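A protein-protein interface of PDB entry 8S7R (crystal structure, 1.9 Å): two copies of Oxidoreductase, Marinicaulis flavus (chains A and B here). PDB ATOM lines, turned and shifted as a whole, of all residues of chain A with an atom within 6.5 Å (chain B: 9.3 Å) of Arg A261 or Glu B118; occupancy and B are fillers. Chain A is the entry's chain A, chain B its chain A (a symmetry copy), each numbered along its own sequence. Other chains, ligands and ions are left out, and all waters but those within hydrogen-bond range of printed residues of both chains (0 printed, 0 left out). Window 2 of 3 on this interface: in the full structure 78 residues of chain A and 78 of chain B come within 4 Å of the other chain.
Among the printed residues, pairs that only touch across the chains: Arg A261 with Phe B119, Ile A396 with Phe B119, Val A265 with Pro B235, Thr A397 with Phe B119 and Val A265 with Glu B118.
NE of Arg A261 lies within salt-bridge range of OE1 of Glu B118, at 3.3 Å.
Hydrophobic or aromatic side chains of chain B within 4 Å of the printed part of chain A: Phe B119 and Pro B235.
Of the 16 printed residues of chain A, 4 touch a printed residue of chain B.
Hydrophobic or aromatic side chains of chain A that line the printed part of chain B: Val A265.
Among the printed residues, 6 pairs touch across the chains.
Among the printed residues, Asp or Glu carboxylates within 4 Å of a Lys or Arg side-chain nitrogen of the other chain: Arg A261 with Glu B118 (3.3 Å).
No position is printed for both chains.
Glu B118 touches two residues of chain A.
No residue of chain B comes within 4 Å of Glu A258.
Printed residues of chain B within 4 Å of Thr A397: Phe B119 (3.8 Å).
Of the printed residues of chain B, Val A265 touches Glu B118 and Pro B235.
Of the printed residues of chain B, Ile A396 touches Phe B119.
Gly B120 touches none of the printed residues of chain A.
The nearest residue of chain A that does not touch Glu B118 is Thr A397 (4.8 Å).
The guanidinium group (NH2) of Arg A261 is in salt-bridge range of the side-chain carboxylate (OE1) of Glu A258 (2.9 Å).
OD1 of Asn B116 is in hydrogen-bond range of N of Phe B119 (3.0 Å).
NE1 of Trp A427 sits at hydrogen-bond distance from O of Val A265, 2.9 Å away.
NH1 of Arg A261 lies within hydrogen-bond range of O of Ile A396.
The side-chain amide oxygen (OD1) of Asn B116 is in hydrogen-bond range of the backbone NH (N) of Glu B118 (3.1 Å).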
ATOM      1  N   VAL A 256       6.386  -9.606   7.395  1.00  0.00           N
ATOM      2  CA  VAL A 256       6.132  -8.792   8.569  1.00  0.00           C
ATOM      3  C   VAL A 256       5.258  -9.547   9.581  1.00  0.00           C
ATOM      4  O   VAL A 256       5.575  -9.530  10.752  1.00  0.00           O
ATOM      5  CB  VAL A 256       5.538  -7.425   8.159  1.00  0.00           C
ATOM      6  CG1 VAL A 256       4.969  -6.670   9.345  1.00  0.00           C
ATOM      7  CG2 VAL A 256       6.585  -6.573   7.461  1.00  0.00           C
ATOM      8  N   THR A 257       4.173 -10.183   9.124  1.00  0.00           N
ATOM      9  CA  THR A 257       3.275 -10.930   9.980  1.00  0.00           C
ATOM     10  C   THR A 257       4.017 -12.107  10.631  1.00  0.00           C
ATOM     11  O   THR A 257       3.891 -12.299  11.826  1.00  0.00           O
ATOM     12  CB  THR A 257       2.043 -11.352   9.176  1.00  0.00           C
ATOM     13  OG1 THR A 257       1.461 -10.181   8.599  1.00  0.00           O
ATOM     14  CG2 THR A 257       1.029 -12.098  10.022  1.00  0.00           C
ATOM     15  N   GLU A 258       4.850 -12.829   9.863  1.00  0.00           N
ATOM     16  CA  GLU A 258       5.668 -13.914  10.386  1.00  0.00           C
ATOM     17  C   GLU A 258       6.519 -13.443  11.566  1.00  0.00           C
ATOM     18  O   GLU A 258       6.623 -14.125  12.593  1.00  0.00           O
ATOM     19  CB  GLU A 258       6.557 -14.506   9.290  1.00  0.00           C
ATOM     20  CG  GLU A 258       5.811 -15.399   8.311  1.00  0.00           C
ATOM     21  CD  GLU A 258       5.243 -16.637   8.982  1.00  0.00           C
ATOM     22  OE1 GLU A 258       6.052 -17.374   9.544  1.00  0.00           O
ATOM     23  OE2 GLU A 258       4.001 -16.846   8.953  1.00  0.00           O
ATOM     24  N   ARG A 259       7.103 -12.253  11.446  1.00  0.00           N
ATOM     25  CA  ARG A 259       8.017 -11.763  12.459  1.00  0.00           C
ATOM     26  C   ARG A 259       7.252 -11.209  13.660  1.00  0.00           C
ATOM     27  O   ARG A 259       7.740 -11.297  14.785  1.00  0.00           O
ATOM     28  CB  ARG A 259       8.945 -10.730  11.823  1.00  0.00           C
ATOM     29  CG  ARG A 259       9.759 -11.285  10.660  1.00  0.00           C
ATOM     30  CD  ARG A 259      10.160 -10.165   9.718  1.00  0.00           C
ATOM     31  NE  ARG A 259      10.881 -10.619   8.536  1.00  0.00           N
ATOM     32  CZ  ARG A 259      12.176 -10.452   8.305  1.00  0.00           C
ATOM     33  NH1 ARG A 259      12.967  -9.902   9.209  1.00  0.00           N
ATOM     34  NH2 ARG A 259      12.683 -10.869   7.160  1.00  0.00           N
ATOM     35  N   LEU A 260       6.053 -10.671  13.417  1.00  0.00           N
ATOM     36  CA  LEU A 260       5.196 -10.152  14.472  1.00  0.00           C
ATOM     37  C   LEU A 260       4.733 -11.280  15.393  1.00  0.00           C
ATOM     38  O   LEU A 260       4.596 -11.047  16.592  1.00  0.00           O
ATOM     39  CB  LEU A 260       3.982  -9.435  13.862  1.00  0.00           C
ATOM     40  CG  LEU A 260       4.225  -8.001  13.364  1.00  0.00           C
ATOM     41  CD1 LEU A 260       2.999  -7.453  12.668  1.00  0.00           C
ATOM     42  CD2 LEU A 260       4.617  -7.073  14.496  1.00  0.00           C
ATOM     43  N   ARG A 261       4.502 -12.482  14.840  1.00  0.00           N
ATOM     44  CA  ARG A 261       3.858 -13.552  15.609  1.00  0.00           C
ATOM     45  C   ARG A 261       4.585 -13.806  16.931  1.00  0.00           C
ATOM     46  O   ARG A 261       3.998 -13.660  17.993  1.00  0.00           O
ATOM     47  CB  ARG A 261       3.757 -14.858  14.824  1.00  0.00           C
ATOM     48  CG  ARG A 261       3.382 -16.059  15.689  1.00  0.00           C
ATOM     49  CD  ARG A 261       3.167 -17.313  14.867  1.00  0.00           C
ATOM     50  NE  ARG A 261       4.383 -17.695  14.170  1.00  0.00           N
ATOM     51  CZ  ARG A 261       4.541 -17.653  12.844  1.00  0.00           C
ATOM     52  NH1 ARG A 261       3.572 -17.238  12.045  1.00  0.00           N
ATOM     53  NH2 ARG A 261       5.678 -18.056  12.305  1.00  0.00           N
ATOM     54  N   PRO A 262       5.883 -14.157  16.952  1.00  0.00           N
ATOM     55  CA  PRO A 262       6.551 -14.450  18.227  1.00  0.00           C
ATOM     56  C   PRO A 262       6.604 -13.257  19.187  1.00  0.00           C
ATOM     57  O   PRO A 262       6.510 -13.442  20.410  1.00  0.00           O
ATOM     58  CB  PRO A 262       7.940 -14.956  17.803  1.00  0.00           C
ATOM     59  CG  PRO A 262       8.116 -14.353  16.415  1.00  0.00           C
ATOM     60  CD  PRO A 262       6.741 -14.433  15.785  1.00  0.00           C
ATOM     61  N   LEU A 263       6.729 -12.035  18.647  1.00  0.00           N
ATOM     62  CA  LEU A 263       6.860 -10.853  19.493  1.00  0.00           C
ATOM     63  C   LEU A 263       5.553 -10.633  20.250  1.00  0.00           C
ATOM     64  O   LEU A 263       5.574 -10.219  21.402  1.00  0.00           O
ATOM     65  CB  LEU A 263       7.195  -9.621  18.634  1.00  0.00           C
ATOM     66  CG  LEU A 263       8.557  -9.623  17.929  1.00  0.00           C
ATOM     67  CD1 LEU A 263       8.656  -8.472  16.927  1.00  0.00           C
ATOM     68  CD2 LEU A 263       9.685  -9.521  18.947  1.00  0.00           C
ATOM     69  N   LYS A 264       4.421 -10.927  19.589  1.00  0.00           N
ATOM     70  CA  LYS A 264       3.106 -10.717  20.171  1.00  0.00           C
ATOM     71  C   LYS A 264       2.732 -11.863  21.109  1.00  0.00           C
ATOM     72  O   LYS A 264       2.283 -11.607  22.217  1.00  0.00           O
ATOM     73  CB  LYS A 264       2.039 -10.547  19.083  1.00  0.00           C
ATOM     74  CG  LYS A 264       1.931  -9.132  18.498  1.00  0.00           C
ATOM     75  CD  LYS A 264       1.563  -8.064  19.469  1.00  0.00           C
ATOM     76  CE  LYS A 264       0.269  -8.324  20.195  1.00  0.00           C
ATOM     77  NZ  LYS A 264       0.142  -7.496  21.404  1.00  0.00           N
ATOM     78  N   VAL A 265       2.960 -13.111  20.694  1.00  0.00           N
ATOM     79  CA  VAL A 265       2.655 -14.244  21.572  1.00  0.00           C
ATOM     80  C   VAL A 265       3.364 -14.106  22.923  1.00  0.00           C
ATOM     81  O   VAL A 265       2.723 -14.260  23.966  1.00  0.00           O
ATOM     82  CB  VAL A 265       2.953 -15.583  20.882  1.00  0.00           C
ATOM     83  CG1 VAL A 265       2.755 -16.758  21.820  1.00  0.00           C
ATOM     84  CG2 VAL A 265       2.088 -15.769  19.664  1.00  0.00           C
ATOM     85  N   ALA A 266       4.670 -13.803  22.899  1.00  0.00           N
ATOM     86  CA  ALA A 266       5.489 -13.618  24.089  1.00  0.00           C
ATOM     87  C   ALA A 266       5.299 -12.258  24.759  1.00  0.00           C
ATOM     88  O   ALA A 266       5.837 -12.046  25.838  1.00  0.00           O
ATOM     89  CB  ALA A 266       6.956 -13.789  23.748  1.00  0.00           C
ATOM     90  N   ILE A 396      -2.020 -15.757  13.125  1.00  0.00           N
ATOM     91  CA  ILE A 396      -0.949 -14.833  12.834  1.00  0.00           C
ATOM     92  C   ILE A 396       0.083 -15.537  11.967  1.00  0.00           C
ATOM     93  O   ILE A 396       1.094 -15.999  12.484  1.00  0.00           O
ATOM     94  CB  ILE A 396      -0.282 -14.262  14.101  1.00  0.00           C
ATOM     95  CG1 ILE A 396      -1.272 -13.733  15.139  1.00  0.00           C
ATOM     96  CG2 ILE A 396       0.721 -13.180  13.717  1.00  0.00           C
ATOM     97  CD1 ILE A 396      -0.627 -13.543  16.481  1.00  0.00           C
ATOM     98  N   THR A 397      -0.208 -15.660  10.664  1.00  0.00           N
ATOM     99  CA  THR A 397       0.775 -16.131   9.696  1.00  0.00           C
ATOM    100  C   THR A 397       0.821 -15.213   8.476  1.00  0.00           C
ATOM    101  O   THR A 397      -0.175 -14.624   8.080  1.00  0.00           O
ATOM    102  CB  THR A 397       0.538 -17.565   9.194  1.00  0.00           C
ATOM    103  OG1 THR A 397      -0.575 -17.580   8.311  1.00  0.00           O
ATOM    104  CG2 THR A 397       0.351 -18.542  10.340  1.00  0.00           C
ATOM    105  N   GLY A 398       2.010 -15.129   7.882  1.00  0.00           N
ATOM    106  CA  GLY A 398       2.202 -14.467   6.602  1.00  0.00           C
ATOM    107  C   GLY A 398       1.222 -14.918   5.535  1.00  0.00           C
ATOM    108  O   GLY A 398       0.681 -14.082   4.811  1.00  0.00           O
ATOM    109  N   ILE A 425      -3.117  -7.205  15.457  1.00  0.00           N
ATOM    110  CA  ILE A 425      -2.881  -8.345  16.335  1.00  0.00           C
ATOM    111  C   ILE A 425      -3.149  -7.949  17.778  1.00  0.00           C
ATOM    112  O   ILE A 425      -2.567  -6.998  18.311  1.00  0.00           O
ATOM    113  CB  ILE A 425      -1.460  -8.916  16.212  1.00  0.00           C
ATOM    114  CG1 ILE A 425      -1.099  -9.279  14.773  1.00  0.00           C
ATOM    115  CG2 ILE A 425      -1.310 -10.109  17.157  1.00  0.00           C
ATOM    116  CD1 ILE A 425       0.374  -9.482  14.538  1.00  0.00           C
ATOM    117  N   TRP A 427      -3.373 -10.477  20.789  1.00  0.00           N
ATOM    118  CA  TRP A 427      -2.357 -11.251  21.486  1.00  0.00           C
ATOM    119  C   TRP A 427      -1.952 -12.441  20.607  1.00  0.00           C
ATOM    120  O   TRP A 427      -0.862 -12.435  20.054  1.00  0.00           O
ATOM    121  CB  TRP A 427      -2.841 -11.646  22.895  1.00  0.00           C
ATOM    122  CG  TRP A 427      -1.810 -12.261  23.799  1.00  0.00           C
ATOM    123  CD1 TRP A 427      -0.508 -12.525  23.496  1.00  0.00           C
ATOM    124  CD2 TRP A 427      -1.984 -12.683  25.171  1.00  0.00           C
ATOM    125  NE1 TRP A 427       0.143 -13.045  24.585  1.00  0.00           N
ATOM    126  CE2 TRP A 427      -0.738 -13.164  25.621  1.00  0.00           C
ATOM    127  CE3 TRP A 427      -3.062 -12.714  26.063  1.00  0.00           C
ATOM    128  CZ2 TRP A 427      -0.565 -13.704  26.892  1.00  0.00           C
ATOM    129  CZ3 TRP A 427      -2.883 -13.218  27.331  1.00  0.00           C
ATOM    130  CH2 TRP A 427      -1.649 -13.706  27.738  1.00  0.00           C
ATOM    131  N   GLU B 114      -3.928 -31.287  20.795  1.00  0.00           N
ATOM    132  CA  GLU B 114      -2.963 -30.467  20.087  1.00  0.00           C
ATOM    133  C   GLU B 114      -2.137 -29.671  21.087  1.00  0.00           C
ATOM    134  O   GLU B 114      -2.641 -29.211  22.123  1.00  0.00           O
ATOM    135  CB  GLU B 114      -3.641 -29.511  19.099  1.00  0.00           C
ATOM    136  CG  GLU B 114      -2.626 -28.760  18.251  1.00  0.00           C
ATOM    137  CD  GLU B 114      -3.091 -27.639  17.331  1.00  0.00           C
ATOM    138  OE1 GLU B 114      -4.303 -27.311  17.313  1.00  0.00           O
ATOM    139  OE2 GLU B 114      -2.214 -27.099  16.623  1.00  0.00           O
ATOM    140  N   VAL B 115      -0.840 -29.562  20.791  1.00  0.00           N
ATOM    141  CA  VAL B 115      -0.005 -28.565  21.418  1.00  0.00           C
ATOM    142  C   VAL B 115       0.684 -27.795  20.298  1.00  0.00           C
ATOM    143  O   VAL B 115       1.431 -28.380  19.534  1.00  0.00           O
ATOM    144  CB  VAL B 115       1.025 -29.114  22.416  1.00  0.00           C
ATOM    145  CG1 VAL B 115       1.785 -27.958  23.066  1.00  0.00           C
ATOM    146  CG2 VAL B 115       0.388 -29.981  23.498  1.00  0.00           C
ATOM    147  N   ASN B 116       0.486 -26.472  20.298  1.00  0.00           N
ATOM    148  CA  ASN B 116       0.939 -25.603  19.232  1.00  0.00           C
ATOM    149  C   ASN B 116       2.010 -24.670  19.765  1.00  0.00           C
ATOM    150  O   ASN B 116       1.756 -23.809  20.602  1.00  0.00           O
ATOM    151  CB  ASN B 116      -0.230 -24.814  18.637  1.00  0.00           C
ATOM    152  CG  ASN B 116       0.170 -24.114  17.361  1.00  0.00           C
ATOM    153  OD1 ASN B 116       1.114 -23.342  17.347  1.00  0.00           O
ATOM    154  ND2 ASN B 116      -0.470 -24.447  16.273  1.00  0.00           N
ATOM    155  N   GLU B 117       3.225 -24.853  19.273  1.00  0.00           N
ATOM    156  CA  GLU B 117       4.353 -24.104  19.781  1.00  0.00           C
ATOM    157  C   GLU B 117       4.330 -22.664  19.235  1.00  0.00           C
ATOM    158  O   GLU B 117       4.559 -21.720  19.986  1.00  0.00           O
ATOM    159  CB  GLU B 117       5.660 -24.802  19.401  1.00  0.00           C
ATOM    160  CG  GLU B 117       6.892 -24.148  20.020  1.00  0.00           C
ATOM    161  CD  GLU B 117       8.217 -24.799  19.629  1.00  0.00           C
ATOM    162  OE1 GLU B 117       8.371 -25.065  18.463  1.00  0.00           O
ATOM    163  OE2 GLU B 117       9.105 -24.983  20.478  1.00  0.00           O
ATOM    164  N   GLU B 118       4.066 -22.475  17.941  1.00  0.00           N
ATOM    165  CA  GLU B 118       4.200 -21.122  17.391  1.00  0.00           C
ATOM    166  C   GLU B 118       3.139 -20.165  17.935  1.00  0.00           C
ATOM    167  O   GLU B 118       3.439 -18.988  18.058  1.00  0.00           O
ATOM    168  CB  GLU B 118       4.220 -21.101  15.866  1.00  0.00           C
ATOM    169  CG  GLU B 118       2.959 -21.595  15.193  1.00  0.00           C
ATOM    170  CD  GLU B 118       3.019 -21.487  13.674  1.00  0.00           C
ATOM    171  OE1 GLU B 118       3.903 -20.771  13.170  1.00  0.00           O
ATOM    172  OE2 GLU B 118       2.185 -22.113  12.994  1.00  0.00           O
ATOM    173  N   PHE B 119       1.945 -20.665  18.302  1.00  0.00           N
ATOM    174  CA  PHE B 119       0.867 -19.857  18.863  1.00  0.00           C
ATOM    175  C   PHE B 119       0.653 -20.060  20.372  1.00  0.00           C
ATOM    176  O   PHE B 119      -0.250 -19.449  20.945  1.00  0.00           O
ATOM    177  CB  PHE B 119      -0.454 -20.166  18.165  1.00  0.00           C
ATOM    178  CG  PHE B 119      -0.447 -19.979  16.667  1.00  0.00           C
ATOM    179  CD1 PHE B 119       0.044 -18.820  16.089  1.00  0.00           C
ATOM    180  CD2 PHE B 119      -0.954 -20.966  15.834  1.00  0.00           C
ATOM    181  CE1 PHE B 119       0.056 -18.668  14.709  1.00  0.00           C
ATOM    182  CE2 PHE B 119      -0.954 -20.803  14.457  1.00  0.00           C
ATOM    183  CZ  PHE B 119      -0.424 -19.663  13.900  1.00  0.00           C
ATOM    184  N   GLY B 120       1.472 -20.903  21.016  1.00  0.00           N
ATOM    185  CA  GLY B 120       1.504 -21.034  22.465  1.00  0.00           C
ATOM    186  C   GLY B 120       0.151 -21.458  23.034  1.00  0.00           C
ATOM    187  O   GLY B 120      -0.464 -20.679  23.748  1.00  0.00           O
ATOM    188  N   TYR B 121      -0.323 -22.662  22.687  1.00  0.00           N
ATOM    189  CA  TYR B 121      -1.556 -23.188  23.249  1.00  0.00           C
ATOM    190  C   TYR B 121      -1.625 -24.722  23.246  1.00  0.00           C
ATOM    191  O   TYR B 121      -0.863 -25.409  22.571  1.00  0.00           O
ATOM    192  CB  TYR B 121      -2.761 -22.623  22.500  1.00  0.00           C
ATOM    193  CG  TYR B 121      -3.060 -23.151  21.124  1.00  0.00           C
ATOM    194  CD1 TYR B 121      -3.653 -24.405  20.944  1.00  0.00           C
ATOM    195  CD2 TYR B 121      -2.810 -22.364  20.003  1.00  0.00           C
ATOM    196  CE1 TYR B 121      -3.959 -24.871  19.681  1.00  0.00           C
ATOM    197  CE2 TYR B 121      -3.137 -22.803  18.727  1.00  0.00           C
ATOM    198  CZ  TYR B 121      -3.711 -24.063  18.574  1.00  0.00           C
ATOM    199  OH  TYR B 121      -4.079 -24.523  17.366  1.00  0.00           O
ATOM    200  N   LEU B 142       9.182 -29.031  22.957  1.00  0.00           N
ATOM    201  CA  LEU B 142       8.510 -27.767  22.646  1.00  0.00           C
ATOM    202  C   LEU B 142       8.870 -26.717  23.697  1.00  0.00           C
ATOM    203  O   LEU B 142       8.861 -27.005  24.891  1.00  0.00           O
ATOM    204  CB  LEU B 142       6.991 -27.985  22.618  1.00  0.00           C
ATOM    205  CG  LEU B 142       6.466 -29.051  21.651  1.00  0.00           C
ATOM    206  CD1 LEU B 142       4.947 -29.052  21.610  1.00  0.00           C
ATOM    207  CD2 LEU B 142       6.992 -28.857  20.241  1.00  0.00           C
ATOM    208  N   LYS B 143       9.110 -25.478  23.253  1.00  0.00           N
ATOM    209  CA  LYS B 143       9.620 -24.396  24.088  1.00  0.00           C
ATOM    210  C   LYS B 143       8.456 -23.652  24.759  1.00  0.00           C
ATOM    211  O   LYS B 143       8.266 -22.444  24.574  1.00  0.00           O
ATOM    212  CB  LYS B 143      10.445 -23.443  23.215  1.00  0.00           C
ATOM    213  CG  LYS B 143      11.629 -24.048  22.465  1.00  0.00           C
ATOM    214  CD  LYS B 143      12.744 -24.485  23.380  1.00  0.00           C
ATOM    215  CE  LYS B 143      13.898 -25.148  22.654  1.00  0.00           C
ATOM    216  NZ  LYS B 143      13.564 -26.536  22.245  1.00  0.00           N
ATOM    217  N   LEU B 144       7.697 -24.386  25.570  1.00  0.00           N
ATOM    218  CA  LEU B 144       6.506 -23.885  26.222  1.00  0.00           C
ATOM    219  C   LEU B 144       6.543 -24.271  27.697  1.00  0.00           C
ATOM    220  O   LEU B 144       7.075 -25.325  28.055  1.00  0.00           O
ATOM    221  CB  LEU B 144       5.286 -24.534  25.558  1.00  0.00           C
ATOM    222  CG  LEU B 144       5.040 -24.243  24.081  1.00  0.00           C
ATOM    223  CD1 LEU B 144       3.824 -25.014  23.598  1.00  0.00           C
ATOM    224  CD2 LEU B 144       4.836 -22.744  23.809  1.00  0.00           C
ATOM    225  N   ASN B 201      -9.304 -22.078  12.236  1.00  0.00           N
ATOM    226  CA  ASN B 201      -8.029 -22.469  12.803  1.00  0.00           C
ATOM    227  C   ASN B 201      -7.720 -21.534  13.973  1.00  0.00           C
ATOM    228  O   ASN B 201      -6.552 -21.331  14.307  1.00  0.00           O
ATOM    229  CB  ASN B 201      -6.943 -22.423  11.727  1.00  0.00           C
ATOM    230  CG  ASN B 201      -7.065 -23.585  10.762  1.00  0.00           C
ATOM    231  OD1 ASN B 201      -6.898 -24.730  11.153  1.00  0.00           O
ATOM    232  ND2 ASN B 201      -7.368 -23.310   9.508  1.00  0.00           N
ATOM    233  N   LEU B 205      -7.193 -19.200  19.596  1.00  0.00           N
ATOM    234  CA  LEU B 205      -6.446 -17.969  19.350  1.00  0.00           C
ATOM    235  C   LEU B 205      -7.241 -16.726  19.771  1.00  0.00           C
ATOM    236  O   LEU B 205      -6.661 -15.654  19.998  1.00  0.00           O
ATOM    237  CB  LEU B 205      -6.108 -17.898  17.860  1.00  0.00           C
ATOM    238  CG  LEU B 205      -5.201 -19.001  17.306  1.00  0.00           C
ATOM    239  CD1 LEU B 205      -4.889 -18.733  15.851  1.00  0.00           C
ATOM    240  CD2 LEU B 205      -3.910 -19.163  18.102  1.00  0.00           C
ATOM    241  N   LEU B 233      -0.577 -21.190  26.704  1.00  0.00           N
ATOM    242  CA  LEU B 233       0.672 -21.642  27.313  1.00  0.00           C
ATOM    243  C   LEU B 233       1.727 -20.563  27.075  1.00  0.00           C
ATOM    244  O   LEU B 233       1.851 -20.069  25.962  1.00  0.00           O
ATOM    245  CB  LEU B 233       1.090 -22.946  26.626  1.00  0.00           C
ATOM    246  CG  LEU B 233       0.133 -24.132  26.809  1.00  0.00           C
ATOM    247  CD1 LEU B 233       0.734 -25.367  26.205  1.00  0.00           C
ATOM    248  CD2 LEU B 233      -0.207 -24.380  28.288  1.00  0.00           C
ATOM    249  N   PRO B 235       5.228 -18.993  26.267  1.00  0.00           N
ATOM    250  CA  PRO B 235       6.511 -19.279  25.632  1.00  0.00           C
ATOM    251  C   PRO B 235       7.601 -19.234  26.679  1.00  0.00           C
ATOM    252  O   PRO B 235       7.598 -18.377  27.576  1.00  0.00           O
ATOM    253  CB  PRO B 235       6.722 -18.167  24.589  1.00  0.00           C
ATOM    254  CG  PRO B 235       5.324 -17.628  24.332  1.00  0.00           C
ATOM    255  CD  PRO B 235       4.543 -17.873  25.609  1.00  0.00           C
